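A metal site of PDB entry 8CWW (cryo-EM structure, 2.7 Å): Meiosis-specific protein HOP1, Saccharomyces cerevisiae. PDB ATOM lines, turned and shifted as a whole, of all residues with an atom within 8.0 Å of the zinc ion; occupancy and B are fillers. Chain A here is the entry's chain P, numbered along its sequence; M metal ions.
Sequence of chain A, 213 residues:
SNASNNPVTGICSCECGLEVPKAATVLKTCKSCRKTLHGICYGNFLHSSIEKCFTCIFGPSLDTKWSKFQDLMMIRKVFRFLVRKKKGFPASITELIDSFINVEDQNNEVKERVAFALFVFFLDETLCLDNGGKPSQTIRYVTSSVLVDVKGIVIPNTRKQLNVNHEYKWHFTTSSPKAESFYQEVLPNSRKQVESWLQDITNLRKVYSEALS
SG of Cys 33 binds the zinc ion, 2.3 Å away. SG of Cys 53 binds the zinc ion (2.3 Å). The side-chain sulfur (SG) of Cys 56 is bound to the zinc ion (2.3 Å). SG of Cys 30 binds the zinc ion, at 2.3 Å.
The side-chain sulfur of Cys 30 lies close to the backbone carbonyl oxygen of Glu 51. The side-chain sulfur of Cys 30 sits close to the backbone NH of Ser 32 (3.8 Å).
Of the 18 residues printed, 4 come within 4 Å of the zinc ion. Along chain A the residues within 4 Å of the zinc ion span positions 30 to 56.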
ATOM      1  N   GLU A  15       0.236 -24.041 -18.459  1.00  0.00           N
ATOM      2  CA  GLU A  15       0.257 -22.620 -18.815  1.00  0.00           C
ATOM      3  C   GLU A  15       1.654 -22.032 -18.683  1.00  0.00           C
ATOM      4  O   GLU A  15       1.944 -21.006 -19.312  1.00  0.00           O
ATOM      5  CB  GLU A  15      -0.736 -21.851 -17.941  1.00  0.00           C
ATOM      6  CG  GLU A  15      -2.200 -22.094 -18.274  1.00  0.00           C
ATOM      7  CD  GLU A  15      -2.701 -23.453 -17.824  1.00  0.00           C
ATOM      8  OE1 GLU A  15      -1.955 -24.150 -17.094  1.00  0.00           O
ATOM      9  OE2 GLU A  15      -3.835 -23.817 -18.190  1.00  0.00           O
ATOM     10  N   THR A  29      -4.079 -33.472 -13.317  1.00  0.00           N
ATOM     11  CA  THR A  29      -4.990 -33.493 -14.459  1.00  0.00           C
ATOM     12  C   THR A  29      -6.201 -32.623 -14.166  1.00  0.00           C
ATOM     13  O   THR A  29      -6.652 -32.521 -13.031  1.00  0.00           O
ATOM     14  CB  THR A  29      -5.435 -34.930 -14.789  1.00  0.00           C
ATOM     15  OG1 THR A  29      -4.296 -35.785 -14.916  1.00  0.00           O
ATOM     16  CG2 THR A  29      -6.206 -34.967 -16.107  1.00  0.00           C
ATOM     17  N   CYS A  30      -6.718 -31.995 -15.221  1.00  0.00           N
ATOM     18  CA  CYS A  30      -7.952 -31.221 -15.162  1.00  0.00           C
ATOM     19  C   CYS A  30      -9.121 -32.092 -15.604  1.00  0.00           C
ATOM     20  O   CYS A  30      -9.001 -32.876 -16.557  1.00  0.00           O
ATOM     21  CB  CYS A  30      -7.872 -29.973 -16.039  1.00  0.00           C
ATOM     22  SG  CYS A  30      -9.306 -28.859 -15.943  1.00  0.00           S
ATOM     23  N   LYS A  31     -10.256 -31.970 -14.904  1.00  0.00           N
ATOM     24  CA  LYS A  31     -11.390 -32.845 -15.185  1.00  0.00           C
ATOM     25  C   LYS A  31     -12.058 -32.492 -16.508  1.00  0.00           C
ATOM     26  O   LYS A  31     -12.496 -33.388 -17.249  1.00  0.00           O
ATOM     27  CB  LYS A  31     -12.397 -32.793 -14.045  1.00  0.00           C
ATOM     28  CG  LYS A  31     -11.964 -33.559 -12.806  1.00  0.00           C
ATOM     29  CD  LYS A  31     -13.051 -33.546 -11.738  1.00  0.00           C
ATOM     30  CE  LYS A  31     -12.627 -34.327 -10.513  1.00  0.00           C
ATOM     31  NZ  LYS A  31     -13.649 -34.264  -9.433  1.00  0.00           N
ATOM     32  N   SER A  32     -12.160 -31.197 -16.820  1.00  0.00           N
ATOM     33  CA  SER A  32     -12.944 -30.789 -17.990  1.00  0.00           C
ATOM     34  C   SER A  32     -12.188 -31.024 -19.295  1.00  0.00           C
ATOM     35  O   SER A  32     -12.623 -31.828 -20.130  1.00  0.00           O
ATOM     36  CB  SER A  32     -13.336 -29.308 -17.854  1.00  0.00           C
ATOM     37  OG  SER A  32     -14.143 -29.096 -16.722  1.00  0.00           O
ATOM     38  N   CYS A  33     -11.068 -30.344 -19.492  1.00  0.00           N
ATOM     39  CA  CYS A  33     -10.331 -30.436 -20.737  1.00  0.00           C
ATOM     40  C   CYS A  33      -9.362 -31.615 -20.784  1.00  0.00           C
ATOM     41  O   CYS A  33      -8.856 -31.926 -21.865  1.00  0.00           O
ATOM     42  CB  CYS A  33      -9.574 -29.130 -21.016  1.00  0.00           C
ATOM     43  SG  CYS A  33      -8.727 -28.442 -19.582  1.00  0.00           S
ATOM     44  N   ARG A  34      -9.098 -32.260 -19.645  1.00  0.00           N
ATOM     45  CA  ARG A  34      -8.322 -33.503 -19.591  1.00  0.00           C
ATOM     46  C   ARG A  34      -6.924 -33.319 -20.203  1.00  0.00           C
ATOM     47  O   ARG A  34      -6.566 -33.957 -21.195  1.00  0.00           O
ATOM     48  CB  ARG A  34      -9.081 -34.641 -20.264  1.00  0.00           C
ATOM     49  CG  ARG A  34     -10.490 -34.839 -19.737  1.00  0.00           C
ATOM     50  CD  ARG A  34     -11.206 -35.957 -20.467  1.00  0.00           C
ATOM     51  NE  ARG A  34     -10.501 -37.227 -20.345  1.00  0.00           N
ATOM     52  CZ  ARG A  34     -10.661 -38.079 -19.333  1.00  0.00           C
ATOM     53  NH1 ARG A  34     -11.493 -37.814 -18.342  1.00  0.00           N
ATOM     54  NH2 ARG A  34      -9.962 -39.207 -19.324  1.00  0.00           N
ATOM     55  N   LYS A  35      -6.139 -32.443 -19.581  1.00  0.00           N
ATOM     56  CA  LYS A  35      -4.774 -32.188 -20.018  1.00  0.00           C
ATOM     57  C   LYS A  35      -3.835 -32.236 -18.820  1.00  0.00           C
ATOM     58  O   LYS A  35      -4.215 -31.936 -17.694  1.00  0.00           O
ATOM     59  CB  LYS A  35      -4.657 -30.827 -20.731  1.00  0.00           C
ATOM     60  CG  LYS A  35      -5.174 -29.643 -19.940  1.00  0.00           C
ATOM     61  CD  LYS A  35      -4.966 -28.351 -20.717  1.00  0.00           C
ATOM     62  CE  LYS A  35      -5.387 -27.142 -19.914  1.00  0.00           C
ATOM     63  NZ  LYS A  35      -5.161 -25.868 -20.655  1.00  0.00           N
ATOM     64  N   LEU A  37      -1.043 -31.373 -16.146  1.00  0.00           N
ATOM     65  CA  LEU A  37      -0.694 -30.146 -15.446  1.00  0.00           C
ATOM     66  C   LEU A  37       0.454 -30.417 -14.496  1.00  0.00           C
ATOM     67  O   LEU A  37       0.679 -31.553 -14.069  1.00  0.00           O
ATOM     68  CB  LEU A  37      -1.895 -29.577 -14.675  1.00  0.00           C
ATOM     69  CG  LEU A  37      -3.139 -29.226 -15.491  1.00  0.00           C
ATOM     70  CD1 LEU A  37      -4.237 -28.706 -14.582  1.00  0.00           C
ATOM     71  CD2 LEU A  37      -2.808 -28.204 -16.568  1.00  0.00           C
ATOM     72  N   TYR A  42       0.394 -25.563  -9.292  1.00  0.00           N
ATOM     73  CA  TYR A  42      -0.941 -25.464  -8.703  1.00  0.00           C
ATOM     74  C   TYR A  42      -0.938 -25.607  -7.188  1.00  0.00           C
ATOM     75  O   TYR A  42      -2.023 -25.656  -6.593  1.00  0.00           O
ATOM     76  CB  TYR A  42      -1.885 -26.493  -9.330  1.00  0.00           C
ATOM     77  CG  TYR A  42      -2.361 -26.105 -10.715  1.00  0.00           C
ATOM     78  CD1 TYR A  42      -1.677 -26.530 -11.846  1.00  0.00           C
ATOM     79  CD2 TYR A  42      -3.482 -25.310 -10.875  1.00  0.00           C
ATOM     80  CE1 TYR A  42      -2.108 -26.177 -13.100  1.00  0.00           C
ATOM     81  CE2 TYR A  42      -3.914 -24.950 -12.136  1.00  0.00           C
ATOM     82  CZ  TYR A  42      -3.227 -25.389 -13.254  1.00  0.00           C
ATOM     83  OH  TYR A  42      -3.665 -25.031 -14.502  1.00  0.00           O
ATOM     84  N   ILE A  50      -8.283 -32.069 -10.793  1.00  0.00           N
ATOM     85  CA  ILE A  50      -8.688 -30.690 -10.530  1.00  0.00           C
ATOM     86  C   ILE A  50      -9.889 -30.368 -11.394  1.00  0.00           C
ATOM     87  O   ILE A  50      -9.924 -30.722 -12.580  1.00  0.00           O
ATOM     88  CB  ILE A  50      -7.530 -29.705 -10.780  1.00  0.00           C
ATOM     89  CG1 ILE A  50      -6.286 -30.135 -10.015  1.00  0.00           C
ATOM     90  CG2 ILE A  50      -7.938 -28.296 -10.375  1.00  0.00           C
ATOM     91  CD1 ILE A  50      -5.101 -29.228 -10.219  1.00  0.00           C
ATOM     92  N   GLU A  51     -10.885 -29.704 -10.808  1.00  0.00           N
ATOM     93  CA  GLU A  51     -12.124 -29.422 -11.524  1.00  0.00           C
ATOM     94  C   GLU A  51     -11.892 -28.486 -12.702  1.00  0.00           C
ATOM     95  O   GLU A  51     -12.311 -28.774 -13.832  1.00  0.00           O
ATOM     96  CB  GLU A  51     -13.165 -28.847 -10.567  1.00  0.00           C
ATOM     97  CG  GLU A  51     -13.528 -29.764  -9.410  1.00  0.00           C
ATOM     98  CD  GLU A  51     -14.591 -29.167  -8.514  1.00  0.00           C
ATOM     99  OE1 GLU A  51     -15.133 -28.095  -8.853  1.00  0.00           O
ATOM    100  OE2 GLU A  51     -14.886 -29.765  -7.458  1.00  0.00           O
ATOM    101  N   LYS A  52     -11.232 -27.351 -12.459  1.00  0.00           N
ATOM    102  CA  LYS A  52     -11.023 -26.356 -13.491  1.00  0.00           C
ATOM    103  C   LYS A  52      -9.621 -25.783 -13.375  1.00  0.00           C
ATOM    104  O   LYS A  52      -9.119 -25.564 -12.268  1.00  0.00           O
ATOM    105  CB  LYS A  52     -12.051 -25.224 -13.399  1.00  0.00           C
ATOM    106  CG  LYS A  52     -13.455 -25.620 -13.806  1.00  0.00           C
ATOM    107  CD  LYS A  52     -14.365 -24.406 -13.915  1.00  0.00           C
ATOM    108  CE  LYS A  52     -15.714 -24.779 -14.506  1.00  0.00           C
ATOM    109  NZ  LYS A  52     -16.587 -23.592 -14.703  1.00  0.00           N
ATOM    110  N   CYS A  53      -8.998 -25.536 -14.523  1.00  0.00           N
ATOM    111  CA  CYS A  53      -7.669 -24.943 -14.590  1.00  0.00           C
ATOM    112  C   CYS A  53      -7.790 -23.458 -14.951  1.00  0.00           C
ATOM    113  O   CYS A  53      -8.887 -22.890 -14.974  1.00  0.00           O
ATOM    114  CB  CYS A  53      -6.799 -25.698 -15.593  1.00  0.00           C
ATOM    115  SG  CYS A  53      -7.453 -25.760 -17.276  1.00  0.00           S
ATOM    116  N   PHE A  54      -6.652 -22.825 -15.225  1.00  0.00           N
ATOM    117  CA  PHE A  54      -6.656 -21.400 -15.561  1.00  0.00           C
ATOM    118  C   PHE A  54      -7.454 -21.134 -16.828  1.00  0.00           C
ATOM    119  O   PHE A  54      -8.220 -20.168 -16.906  1.00  0.00           O
ATOM    120  CB  PHE A  54      -5.232 -20.889 -15.708  1.00  0.00           C
ATOM    121  CG  PHE A  54      -4.505 -20.715 -14.404  1.00  0.00           C
ATOM    122  CD1 PHE A  54      -4.631 -19.536 -13.681  1.00  0.00           C
ATOM    123  CD2 PHE A  54      -3.706 -21.726 -13.908  1.00  0.00           C
ATOM    124  CE1 PHE A  54      -3.968 -19.377 -12.483  1.00  0.00           C
ATOM    125  CE2 PHE A  54      -3.043 -21.574 -12.704  1.00  0.00           C
ATOM    126  CZ  PHE A  54      -3.177 -20.394 -11.992  1.00  0.00           C
ATOM    127  N   THR A  55      -7.279 -21.983 -17.853  1.00  0.00           N
ATOM    128  CA  THR A  55      -7.997 -21.785 -19.113  1.00  0.00           C
ATOM    129  C   THR A  55      -9.505 -21.910 -18.911  1.00  0.00           C
ATOM    130  O   THR A  55     -10.284 -21.123 -19.463  1.00  0.00           O
ATOM    131  CB  THR A  55      -7.498 -22.781 -20.154  1.00  0.00           C
ATOM    132  OG1 THR A  55      -6.084 -22.643 -20.316  1.00  0.00           O
ATOM    133  CG2 THR A  55      -8.182 -22.537 -21.485  1.00  0.00           C
ATOM    134  N   CYS A  56      -9.939 -22.908 -18.138  1.00  0.00           N
ATOM    135  CA  CYS A  56     -11.363 -23.084 -17.885  1.00  0.00           C
ATOM    136  C   CYS A  56     -11.950 -21.890 -17.145  1.00  0.00           C
ATOM    137  O   CYS A  56     -13.044 -21.418 -17.476  1.00  0.00           O
ATOM    138  CB  CYS A  56     -11.611 -24.367 -17.092  1.00  0.00           C
ATOM    139  SG  CYS A  56     -11.087 -25.904 -17.909  1.00  0.00           S
ATOM    140  N   ILE A  57     -11.237 -21.380 -16.129  1.00  0.00           N
ATOM    141  CA  ILE A  57     -11.765 -20.293 -15.319  1.00  0.00           C
ATOM    142  C   ILE A  57     -11.794 -18.985 -16.110  1.00  0.00           C
ATOM    143  O   ILE A  57     -12.793 -18.257 -16.097  1.00  0.00           O
ATOM    144  CB  ILE A  57     -10.954 -20.143 -14.021  1.00  0.00           C
ATOM    145  CG1 ILE A  57     -11.167 -21.368 -13.119  1.00  0.00           C
ATOM    146  CG2 ILE A  57     -11.328 -18.864 -13.296  1.00  0.00           C
ATOM    147  CD1 ILE A  57     -10.479 -21.262 -11.779  1.00  0.00           C
HETATM  148 ZN    ZN M   1      -9.194 -27.254 -17.645  1.00  0.00          ZN
